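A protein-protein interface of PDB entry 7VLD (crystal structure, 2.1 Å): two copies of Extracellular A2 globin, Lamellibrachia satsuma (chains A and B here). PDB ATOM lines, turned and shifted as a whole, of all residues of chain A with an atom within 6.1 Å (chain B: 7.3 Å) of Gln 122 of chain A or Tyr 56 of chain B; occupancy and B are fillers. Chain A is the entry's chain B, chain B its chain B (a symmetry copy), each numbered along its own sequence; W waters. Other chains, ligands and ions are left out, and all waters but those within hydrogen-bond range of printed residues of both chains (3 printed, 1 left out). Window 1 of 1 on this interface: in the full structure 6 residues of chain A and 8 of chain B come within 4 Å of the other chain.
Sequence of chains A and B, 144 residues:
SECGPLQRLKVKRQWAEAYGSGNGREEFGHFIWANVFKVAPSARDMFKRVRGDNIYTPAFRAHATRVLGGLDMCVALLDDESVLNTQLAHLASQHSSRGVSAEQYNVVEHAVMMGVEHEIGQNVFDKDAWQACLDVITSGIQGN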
ATOM      1  N   MET A 114       3.180 -15.749  22.846  1.00  0.00           N
ATOM      2  CA  MET A 114       4.088 -16.617  22.103  1.00  0.00           C
ATOM      3  C   MET A 114       3.437 -17.964  21.813  1.00  0.00           C
ATOM      4  O   MET A 114       3.630 -18.536  20.733  1.00  0.00           O
ATOM      5  CB  MET A 114       5.397 -16.808  22.873  1.00  0.00           C
ATOM      6  CG  MET A 114       6.195 -15.530  23.090  1.00  0.00           C
ATOM      7  SD  MET A 114       6.515 -14.594  21.580  1.00  0.00           S
ATOM      8  CE  MET A 114       7.584 -15.721  20.688  1.00  0.00           C
ATOM      9  N   GLU A 117       0.855 -17.409  18.926  1.00  0.00           N
ATOM     10  CA  GLU A 117       1.575 -17.224  17.670  1.00  0.00           C
ATOM     11  C   GLU A 117       2.218 -18.524  17.206  1.00  0.00           C
ATOM     12  O   GLU A 117       2.186 -18.850  16.015  1.00  0.00           O
ATOM     13  CB  GLU A 117       2.637 -16.135  17.821  1.00  0.00           C
ATOM     14  CG  GLU A 117       3.436 -15.897  16.548  1.00  0.00           C
ATOM     15  CD  GLU A 117       4.904 -15.632  16.809  1.00  0.00           C
ATOM     16  OE1 GLU A 117       5.227 -15.024  17.851  1.00  0.00           O
ATOM     17  OE2 GLU A 117       5.738 -16.039  15.973  1.00  0.00           O
ATOM     18  N   HIS A 118       2.809 -19.279  18.136  1.00  0.00           N
ATOM     19  CA  HIS A 118       3.415 -20.557  17.782  1.00  0.00           C
ATOM     20  C   HIS A 118       2.382 -21.530  17.228  1.00  0.00           C
ATOM     21  O   HIS A 118       2.715 -22.387  16.399  1.00  0.00           O
ATOM     22  CB  HIS A 118       4.124 -21.145  19.005  1.00  0.00           C
ATOM     23  CG  HIS A 118       4.113 -22.641  19.064  1.00  0.00           C
ATOM     24  ND1 HIS A 118       5.005 -23.424  18.363  1.00  0.00           N
ATOM     25  CD2 HIS A 118       3.325 -23.498  19.756  1.00  0.00           C
ATOM     26  CE1 HIS A 118       4.762 -24.697  18.615  1.00  0.00           C
ATOM     27  NE2 HIS A 118       3.748 -24.770  19.457  1.00  0.00           N
ATOM     28  N   ILE A 120      -0.726 -20.593  15.649  1.00  0.00           N
ATOM     29  CA  ILE A 120      -1.393 -20.121  14.442  1.00  0.00           C
ATOM     30  C   ILE A 120      -0.435 -19.499  13.431  1.00  0.00           C
ATOM     31  O   ILE A 120      -0.817 -19.346  12.261  1.00  0.00           O
ATOM     32  CB  ILE A 120      -2.529 -19.131  14.778  1.00  0.00           C
ATOM     33  CG1 ILE A 120      -1.959 -17.792  15.248  1.00  0.00           C
ATOM     34  CG2 ILE A 120      -3.450 -19.722  15.834  1.00  0.00           C
ATOM     35  CD1 ILE A 120      -3.020 -16.757  15.560  1.00  0.00           C
ATOM     36  N   GLY A 121       0.774 -19.137  13.831  1.00  0.00           N
ATOM     37  CA  GLY A 121       1.773 -18.644  12.898  1.00  0.00           C
ATOM     38  C   GLY A 121       2.023 -17.153  13.041  1.00  0.00           C
ATOM     39  O   GLY A 121       1.093 -16.359  13.235  1.00  0.00           O
ATOM     40  N   GLN A 122       3.299 -16.764  12.940  1.00  0.00           N
ATOM     41  CA  GLN A 122       3.659 -15.350  12.917  1.00  0.00           C
ATOM     42  C   GLN A 122       2.992 -14.613  11.767  1.00  0.00           C
ATOM     43  O   GLN A 122       2.810 -13.392  11.842  1.00  0.00           O
ATOM     44  CB  GLN A 122       5.181 -15.195  12.821  1.00  0.00           C
ATOM     45  CG  GLN A 122       5.811 -15.806  11.563  1.00  0.00           C
ATOM     46  CD  GLN A 122       5.755 -14.881  10.357  1.00  0.00           C
ATOM     47  OE1 GLN A 122       5.730 -13.658  10.498  1.00  0.00           O
ATOM     48  NE2 GLN A 122       5.727 -15.464   9.164  1.00  0.00           N
ATOM     49  N   ASN A 123       2.623 -15.339  10.708  1.00  0.00           N
ATOM     50  CA  ASN A 123       2.058 -14.726   9.513  1.00  0.00           C
ATOM     51  C   ASN A 123       0.747 -14.006   9.802  1.00  0.00           C
ATOM     52  O   ASN A 123       0.435 -13.003   9.149  1.00  0.00           O
ATOM     53  CB  ASN A 123       1.859 -15.806   8.447  1.00  0.00           C
ATOM     54  CG  ASN A 123       1.238 -15.272   7.177  1.00  0.00           C
ATOM     55  OD1 ASN A 123       1.636 -14.226   6.664  1.00  0.00           O
ATOM     56  ND2 ASN A 123       0.247 -15.990   6.660  1.00  0.00           N
ATOM     57  N   VAL A 124      -0.027 -14.489  10.771  1.00  0.00           N
ATOM     58  CA  VAL A 124      -1.351 -13.939  11.046  1.00  0.00           C
ATOM     59  C   VAL A 124      -1.490 -13.374  12.450  1.00  0.00           C
ATOM     60  O   VAL A 124      -2.488 -12.686  12.722  1.00  0.00           O
ATOM     61  CB  VAL A 124      -2.459 -14.985  10.795  1.00  0.00           C
ATOM     62  CG1 VAL A 124      -2.408 -15.484   9.359  1.00  0.00           C
ATOM     63  CG2 VAL A 124      -2.330 -16.139  11.776  1.00  0.00           C
ATOM     64  N   PHE A 125      -0.544 -13.632  13.351  1.00  0.00           N
ATOM     65  CA  PHE A 125      -0.698 -13.212  14.739  1.00  0.00           C
ATOM     66  C   PHE A 125      -0.821 -11.695  14.836  1.00  0.00           C
ATOM     67  O   PHE A 125       0.013 -10.954  14.309  1.00  0.00           O
ATOM     68  CB  PHE A 125       0.482 -13.703  15.578  1.00  0.00           C
ATOM     69  CG  PHE A 125       0.376 -13.353  17.035  1.00  0.00           C
ATOM     70  CD1 PHE A 125      -0.548 -13.990  17.848  1.00  0.00           C
ATOM     71  CD2 PHE A 125       1.201 -12.391  17.594  1.00  0.00           C
ATOM     72  CE1 PHE A 125      -0.650 -13.671  19.189  1.00  0.00           C
ATOM     73  CE2 PHE A 125       1.104 -12.070  18.937  1.00  0.00           C
ATOM     74  CZ  PHE A 125       0.178 -12.709  19.734  1.00  0.00           C
ATOM     75  N   ASP A 126      -1.879 -11.240  15.505  1.00  0.00           N
ATOM     76  CA  ASP A 126      -2.159  -9.817  15.694  1.00  0.00           C
ATOM     77  C   ASP A 126      -1.666  -9.441  17.089  1.00  0.00           C
ATOM     78  O   ASP A 126      -2.378  -9.591  18.082  1.00  0.00           O
ATOM     79  CB  ASP A 126      -3.649  -9.535  15.515  1.00  0.00           C
ATOM     80  CG  ASP A 126      -3.964  -8.050  15.404  1.00  0.00           C
ATOM     81  OD1 ASP A 126      -3.285  -7.232  16.060  1.00  0.00           O
ATOM     82  OD2 ASP A 126      -4.905  -7.703  14.659  1.00  0.00           O
ATOM     83  N   LYS A 127      -0.428  -8.942  17.154  1.00  0.00           N
ATOM     84  CA  LYS A 127       0.186  -8.638  18.444  1.00  0.00           C
ATOM     85  C   LYS A 127      -0.540  -7.505  19.161  1.00  0.00           C
ATOM     86  O   LYS A 127      -0.759  -7.577  20.376  1.00  0.00           O
ATOM     87  CB  LYS A 127       1.662  -8.287  18.252  1.00  0.00           C
ATOM     88  CG  LYS A 127       2.343  -7.761  19.510  1.00  0.00           C
ATOM     89  CD  LYS A 127       3.771  -7.321  19.226  1.00  0.00           C
ATOM     90  CE  LYS A 127       4.450  -6.798  20.483  1.00  0.00           C
ATOM     91  NZ  LYS A 127       3.748  -5.612  21.048  1.00  0.00           N
ATOM     92  N   GLU B  26       9.308 -13.573   4.159  1.00  0.00           N
ATOM     93  CA  GLU B  26       8.657 -12.983   5.324  1.00  0.00           C
ATOM     94  C   GLU B  26       9.039 -13.728   6.597  1.00  0.00           C
ATOM     95  O   GLU B  26       9.430 -13.114   7.596  1.00  0.00           O
ATOM     96  CB  GLU B  26       7.141 -12.979   5.142  1.00  0.00           C
ATOM     97  CG  GLU B  26       6.402 -12.266   6.261  1.00  0.00           C
ATOM     98  CD  GLU B  26       4.910 -12.527   6.237  1.00  0.00           C
ATOM     99  OE1 GLU B  26       4.490 -13.621   6.671  1.00  0.00           O
ATOM    100  OE2 GLU B  26       4.160 -11.640   5.779  1.00  0.00           O
ATOM    101  N   GLU B  27       8.924 -15.059   6.581  1.00  0.00           N
ATOM    102  CA  GLU B  27       9.313 -15.852   7.741  1.00  0.00           C
ATOM    103  C   GLU B  27      10.805 -15.723   8.016  1.00  0.00           C
ATOM    104  O   GLU B  27      11.226 -15.643   9.176  1.00  0.00           O
ATOM    105  CB  GLU B  27       8.924 -17.317   7.523  1.00  0.00           C
ATOM    106  CG  GLU B  27       9.153 -18.233   8.721  1.00  0.00           C
ATOM    107  CD  GLU B  27      10.586 -18.721   8.832  1.00  0.00           C
ATOM    108  OE1 GLU B  27      11.035 -18.998   9.965  1.00  0.00           O
ATOM    109  OE2 GLU B  27      11.264 -18.823   7.788  1.00  0.00           O
ATOM    110  N   PHE B  28      11.619 -15.708   6.957  1.00  0.00           N
ATOM    111  CA  PHE B  28      13.062 -15.546   7.108  1.00  0.00           C
ATOM    112  C   PHE B  28      13.391 -14.268   7.870  1.00  0.00           C
ATOM    113  O   PHE B  28      14.129 -14.292   8.862  1.00  0.00           O
ATOM    114  CB  PHE B  28      13.721 -15.547   5.726  1.00  0.00           C
ATOM    115  CG  PHE B  28      15.225 -15.542   5.760  1.00  0.00           C
ATOM    116  CD1 PHE B  28      15.920 -16.156   6.788  1.00  0.00           C
ATOM    117  CD2 PHE B  28      15.945 -14.920   4.751  1.00  0.00           C
ATOM    118  CE1 PHE B  28      17.305 -16.147   6.810  1.00  0.00           C
ATOM    119  CE2 PHE B  28      17.327 -14.907   4.769  1.00  0.00           C
ATOM    120  CZ  PHE B  28      18.008 -15.521   5.798  1.00  0.00           C
ATOM    121  N   GLY B  29      12.833 -13.139   7.427  1.00  0.00           N
ATOM    122  CA  GLY B  29      13.099 -11.876   8.091  1.00  0.00           C
ATOM    123  C   GLY B  29      12.512 -11.790   9.485  1.00  0.00           C
ATOM    124  O   GLY B  29      13.083 -11.134  10.361  1.00  0.00           O
ATOM    125  N   HIS B  30      11.367 -12.440   9.713  1.00  0.00           N
ATOM    126  CA  HIS B  30      10.774 -12.428  11.047  1.00  0.00           C
ATOM    127  C   HIS B  30      11.640 -13.189  12.043  1.00  0.00           C
ATOM    128  O   HIS B  30      11.846 -12.729  13.172  1.00  0.00           O
ATOM    129  CB  HIS B  30       9.369 -13.023  11.017  1.00  0.00           C
ATOM    130  CG  HIS B  30       8.749 -13.153  12.371  1.00  0.00           C
ATOM    131  ND1 HIS B  30       8.111 -12.106  13.001  1.00  0.00           N
ATOM    132  CD2 HIS B  30       8.688 -14.201  13.228  1.00  0.00           C
ATOM    133  CE1 HIS B  30       7.673 -12.507  14.183  1.00  0.00           C
ATOM    134  NE2 HIS B  30       8.011 -13.773  14.345  1.00  0.00           N
ATOM    135  N   PHE B  31      12.142 -14.362  11.646  1.00  0.00           N
ATOM    136  CA  PHE B  31      13.006 -15.141  12.528  1.00  0.00           C
ATOM    137  C   PHE B  31      14.242 -14.346  12.927  1.00  0.00           C
ATOM    138  O   PHE B  31      14.669 -14.386  14.086  1.00  0.00           O
ATOM    139  CB  PHE B  31      13.404 -16.449  11.841  1.00  0.00           C
ATOM    140  CG  PHE B  31      14.165 -17.399  12.726  1.00  0.00           C
ATOM    141  CD1 PHE B  31      15.536 -17.274  12.893  1.00  0.00           C
ATOM    142  CD2 PHE B  31      13.510 -18.433  13.377  1.00  0.00           C
ATOM    143  CE1 PHE B  31      16.235 -18.148  13.703  1.00  0.00           C
ATOM    144  CE2 PHE B  31      14.205 -19.313  14.187  1.00  0.00           C
ATOM    145  CZ  PHE B  31      15.569 -19.171  14.349  1.00  0.00           C
ATOM    146  N   ALA B  34      13.156 -11.209  15.301  1.00  0.00           N
ATOM    147  CA  ALA B  34      12.735 -11.686  16.613  1.00  0.00           C
ATOM    148  C   ALA B  34      13.937 -12.075  17.462  1.00  0.00           C
ATOM    149  O   ALA B  34      13.910 -11.921  18.688  1.00  0.00           O
ATOM    150  CB  ALA B  34      11.777 -12.867  16.466  1.00  0.00           C
ATOM    151  N   ARG B  44      15.237  -1.632  20.011  1.00  0.00           N
ATOM    152  CA  ARG B  44      13.958  -1.346  19.365  1.00  0.00           C
ATOM    153  C   ARG B  44      13.700   0.150  19.243  1.00  0.00           C
ATOM    154  O   ARG B  44      13.011   0.584  18.314  1.00  0.00           O
ATOM    155  CB  ARG B  44      12.817  -2.012  20.136  1.00  0.00           C
ATOM    156  CG  ARG B  44      13.115  -3.434  20.572  1.00  0.00           C
ATOM    157  CD  ARG B  44      11.914  -4.100  21.219  1.00  0.00           C
ATOM    158  NE  ARG B  44      11.163  -4.895  20.255  1.00  0.00           N
ATOM    159  CZ  ARG B  44      10.279  -5.831  20.582  1.00  0.00           C
ATOM    160  NH1 ARG B  44      10.032  -6.099  21.857  1.00  0.00           N
ATOM    161  NH2 ARG B  44       9.646  -6.505  19.632  1.00  0.00           N
ATOM    162  N   ARG B  51       7.964   0.973  13.387  1.00  0.00           N
ATOM    163  CA  ARG B  51       7.220   0.145  14.337  1.00  0.00           C
ATOM    164  C   ARG B  51       8.070  -1.011  14.864  1.00  0.00           C
ATOM    165  O   ARG B  51       7.688  -2.181  14.787  1.00  0.00           O
ATOM    166  CB  ARG B  51       5.918  -0.372  13.715  1.00  0.00           C
ATOM    167  CG  ARG B  51       4.921   0.715  13.337  1.00  0.00           C
ATOM    168  CD  ARG B  51       4.369   1.424  14.565  1.00  0.00           C
ATOM    169  NE  ARG B  51       3.987   0.486  15.616  1.00  0.00           N
ATOM    170  CZ  ARG B  51       2.845  -0.195  15.637  1.00  0.00           C
ATOM    171  NH1 ARG B  51       1.964  -0.050  14.657  1.00  0.00           N
ATOM    172  NH2 ARG B  51       2.587  -1.026  16.637  1.00  0.00           N
ATOM    173  N   ASP B  53       8.359  -1.663  17.802  1.00  0.00           N
ATOM    174  CA  ASP B  53       7.602  -2.234  18.908  1.00  0.00           C
ATOM    175  C   ASP B  53       6.789  -3.448  18.486  1.00  0.00           C
ATOM    176  O   ASP B  53       6.418  -4.260  19.342  1.00  0.00           O
ATOM    177  CB  ASP B  53       6.663  -1.180  19.497  1.00  0.00           C
ATOM    178  CG  ASP B  53       5.702  -0.621  18.464  1.00  0.00           C
ATOM    179  OD1 ASP B  53       6.174  -0.088  17.438  1.00  0.00           O
ATOM    180  OD2 ASP B  53       4.475  -0.724  18.671  1.00  0.00           O
ATOM    181  N   ASN B  54       6.501  -3.589  17.191  1.00  0.00           N
ATOM    182  CA  ASN B  54       5.607  -4.642  16.703  1.00  0.00           C
ATOM    183  C   ASN B  54       6.116  -5.084  15.329  1.00  0.00           C
ATOM    184  O   ASN B  54       5.759  -4.493  14.306  1.00  0.00           O
ATOM    185  CB  ASN B  54       4.170  -4.145  16.639  1.00  0.00           C
ATOM    186  CG  ASN B  54       3.178  -5.251  16.331  1.00  0.00           C
ATOM    187  OD1 ASN B  54       3.553  -6.347  15.922  1.00  0.00           O
ATOM    188  ND2 ASN B  54       1.895  -4.959  16.521  1.00  0.00           N
ATOM    189  N   ILE B  55       6.921  -6.148  15.315  1.00  0.00           N
ATOM    190  CA  ILE B  55       7.556  -6.615  14.089  1.00  0.00           C
ATOM    191  C   ILE B  55       6.563  -7.391  13.219  1.00  0.00           C
ATOM    192  O   ILE B  55       6.914  -7.865  12.136  1.00  0.00           O
ATOM    193  CB  ILE B  55       8.796  -7.477  14.398  1.00  0.00           C
ATOM    194  CG1 ILE B  55       8.396  -8.790  15.071  1.00  0.00           C
ATOM    195  CG2 ILE B  55       9.782  -6.709  15.252  1.00  0.00           C
ATOM    196  CD1 ILE B  55       9.563  -9.729  15.297  1.00  0.00           C
ATOM    197  N   TYR B  56       5.324  -7.528  13.693  1.00  0.00           N
ATOM    198  CA  TYR B  56       4.278  -8.180  12.909  1.00  0.00           C
ATOM    199  C   TYR B  56       3.548  -7.217  11.978  1.00  0.00           C
ATOM    200  O   TYR B  56       2.783  -7.667  11.119  1.00  0.00           O
ATOM    201  CB  TYR B  56       3.256  -8.861  13.832  1.00  0.00           C
ATOM    202  CG  TYR B  56       3.853  -9.895  14.761  1.00  0.00           C
ATOM    203  CD1 TYR B  56       4.383  -9.525  15.990  1.00  0.00           C
ATOM    204  CD2 TYR B  56       3.890 -11.240  14.410  1.00  0.00           C
ATOM    205  CE1 TYR B  56       4.935 -10.464  16.844  1.00  0.00           C
ATOM    206  CE2 TYR B  56       4.440 -12.185  15.257  1.00  0.00           C
ATOM    207  CZ  TYR B  56       4.961 -11.789  16.472  1.00  0.00           C
ATOM    208  OH  TYR B  56       5.509 -12.720  17.322  1.00  0.00           O
ATOM    209  N   THR B  57       3.777  -5.916  12.128  1.00  0.00           N
ATOM    210  CA  THR B  57       3.082  -4.921  11.330  1.00  0.00           C
ATOM    211  C   THR B  57       3.648  -4.872   9.912  1.00  0.00           C
ATOM    212  O   THR B  57       4.820  -5.183   9.692  1.00  0.00           O
ATOM    213  CB  THR B  57       3.216  -3.543  11.973  1.00  0.00           C
ATOM    214  OG1 THR B  57       4.601  -3.181  12.035  1.00  0.00           O
ATOM    215  CG2 THR B  57       2.638  -3.551  13.376  1.00  0.00           C
ATOM    216  N   PRO B  58       2.834  -4.470   8.932  1.00  0.00           N
ATOM    217  CA  PRO B  58       3.373  -4.265   7.577  1.00  0.00           C
ATOM    218  C   PRO B  58       4.493  -3.242   7.526  1.00  0.00           C
ATOM    219  O   PRO B  58       5.369  -3.335   6.656  1.00  0.00           O
ATOM    220  CB  PRO B  58       2.146  -3.799   6.779  1.00  0.00           C
ATOM    221  CG  PRO B  58       0.975  -4.331   7.538  1.00  0.00           C
ATOM    222  CD  PRO B  58       1.373  -4.286   8.983  1.00  0.00           C
ATOM    223  N   ALA B  59       4.497  -2.271   8.442  1.00  0.00           N
ATOM    224  CA  ALA B  59       5.532  -1.244   8.440  1.00  0.00           C
ATOM    225  C   ALA B  59       6.901  -1.834   8.751  1.00  0.00           C
ATOM    226  O   ALA B  59       7.889  -1.521   8.077  1.00  0.00           O
ATOM    227  CB  ALA B  59       5.181  -0.140   9.439  1.00  0.00           C
ATOM    228  N   PHE B  60       6.984  -2.692   9.771  1.00  0.00           N
ATOM    229  CA  PHE B  60       8.276  -3.290  10.094  1.00  0.00           C
ATOM    230  C   PHE B  60       8.655  -4.374   9.097  1.00  0.00           C
ATOM    231  O   PHE B  60       9.837  -4.533   8.773  1.00  0.00           O
ATOM    232  CB  PHE B  60       8.280  -3.864  11.511  1.00  0.00           C
ATOM    233  CG  PHE B  60       9.638  -4.329  11.959  1.00  0.00           C
ATOM    234  CD1 PHE B  60      10.514  -3.450  12.574  1.00  0.00           C
ATOM    235  CD2 PHE B  60      10.052  -5.631  11.733  1.00  0.00           C
ATOM    236  CE1 PHE B  60      11.771  -3.868  12.974  1.00  0.00           C
ATOM    237  CE2 PHE B  60      11.308  -6.055  12.129  1.00  0.00           C
ATOM    238  CZ  PHE B  60      12.167  -5.172  12.751  1.00  0.00           C
ATOM    239  N   ARG B  61       7.671  -5.139   8.613  1.00  0.00           N
ATOM    240  CA  ARG B  61       7.964  -6.167   7.620  1.00  0.00           C
ATOM    241  C   ARG B  61       8.574  -5.568   6.362  1.00  0.00           C
ATOM    242  O   ARG B  61       9.389  -6.217   5.696  1.00  0.00           O
ATOM    243  CB  ARG B  61       6.696  -6.952   7.282  1.00  0.00           C
ATOM    244  CG  ARG B  61       6.127  -7.748   8.448  1.00  0.00           C
ATOM    245  CD  ARG B  61       4.927  -8.581   8.019  1.00  0.00           C
ATOM    246  NE  ARG B  61       4.267  -9.225   9.152  1.00  0.00           N
ATOM    247  CZ  ARG B  61       4.673 -10.364   9.707  1.00  0.00           C
ATOM    248  NH1 ARG B  61       4.007 -10.876  10.732  1.00  0.00           N
ATOM    249  NH2 ARG B  61       5.746 -10.987   9.241  1.00  0.00           N
HETATM  250  O   HOH W   1       1.995 -11.247   7.668  1.00  0.00           O
HETATM  251  O   HOH W   2       8.120 -14.956  16.716  1.00  0.00           O
HETATM  252  O   HOH W   3      -0.060  -6.918  15.145  1.00  0.00           O
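Water W2 lies within hydrogen-bond range of a ring nitrogen (NE2) of His 30 of chain B, the side-chain carboxylate of Glu 117 of chain A and the side-chain hydroxyl of Tyr 56 of chain B. Water W1 lies within hydrogen-bond range of O of Asn 123 of chain A, OE2 of Glu 26 of chain B and NE of Arg 61 of chain B. Water W3 lies within hydrogen-bond range of the backbone NH (N) of Lys 127 of chain A (2.9 Å), the side-chain amide nitrogen (ND2) of Asn 54 of chain B (3.1 Å) and the side-chain carboxylate (OD1) of Asp 126 of chain A (3.4 Å).
Of the printed residues of chain B, Gln 122 of chain A touches Glu 26 (3.3 Å), Glu 27 (3.9 Å), His 30 (3.5 Å), Tyr 56 (3.5 Å) and Arg 61 (3.0 Å). Tyr 56 of chain B touches just these residues of chain A: Glu 117 (2.4 Å), Gln 122 (3.5 Å), Phe 125 (3.9 Å) and Lys 127 (3.7 Å). Printed residues of chain A within 4 Å of His 30 of chain B: Glu 117 and Gln 122. Of the printed residues of chain B, Phe 125 of chain A touches Tyr 56. Of the printed residues of chain B, Glu 117 of chain A touches His 30 and Tyr 56. Printed residues of chain A within 4 Å of Glu 26 of chain B: Gln 122 (3.3 Å) and Asn 123 (2.9 Å). Arg 51 of chain B touches none of the printed residues of chain A. Pro 58 of chain B touches none of the printed residues of chain A. The nearest residue of chain B that does not touch Gln 122 of chain A is Ile 55 of chain B (6.1 Å).
The backbone carbonyl oxygen (O) of Asp 53 of chain B sits close to the side-chain amino group (NZ) of Lys 127 of chain A, 3.4 Å away. The side-chain carboxylate (OE1) of Glu 26 of chain B is in hydrogen-bond range of the side-chain amide nitrogen (NE2) of Gln 122 of chain A, at 3.3 Å. The guanidinium group (NH2) of Arg 61 of chain B lies within hydrogen-bond range of the side-chain amide oxygen (OE1) of Gln 122 of chain A, at 3.0 Å. The side-chain carboxylate (OE1) of Glu 117 of chain A lies close to the side-chain hydroxyl (OH) of Tyr 56 of chain B, at 2.4 Å. OE1 of Glu 26 of chain B lies close to OD1 of Asn 123 of chain A, at 2.9 Å.
Of the 18 printed residues of chain B, 7 touch a printed residue of chain A. Hydrophobic or aromatic side chains of chain B that line the printed part of chain A: His 30 and Tyr 56. Along chain B the printed residues that touch a printed residue of chain A span positions 26 to 61. Of the 11 printed residues of chain A, 5 touch a printed residue of chain B. Printed residues of chain A that touch a printed residue of chain B: Glu 117, Gln 122, Asn 123, Phe 125 and Lys 127. Hydrophobic or aromatic side chains of chain A that line the printed part of chain B: Phe 125. Among the printed residues, 12 pairs touch across the chains.
No position is printed for both chains.
Among the printed residues, merely in contact across the chains: Lys 127 of chain A with Asn 54 of chain B (3.5 Å), Gln 122 of chain A with His 30 of chain B (3.5 Å), Gln 122 of chain A with Tyr 56 of chain B (3.5 Å), Glu 117 of chain A with His 30 of chain B (3.6 Å), Lys 127 of chain A with Tyr 56 of chain B (3.7 Å), Gln 122 of chain A with Glu 27 of chain B (3.9 Å) and Phe 125 of chain A with Tyr 56 of chain B (3.9 Å).
OD2 of Asp 53 of chain B is in salt-bridge range of NH2 of Arg 51 of chain B (2.8 Å). O of Tyr 56 of chain B is in hydrogen-bond range of NE of Arg 61 of chain B. The side-chain hydroxyl (OG1) of Thr 57 of chain B lies within hydrogen-bond range of the backbone carbonyl oxygen (O) of Asn 54 of chain B (2.9 Å). The guanidinium group (NH2) of Arg 61 of chain B lies within salt-bridge range of the side-chain carboxylate (OE2) of Glu 26 of chain B, at 3.9 Å. N of Tyr 56 of chain B lies close to OD1 of Asn 54 of chain B (3.1 Å).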
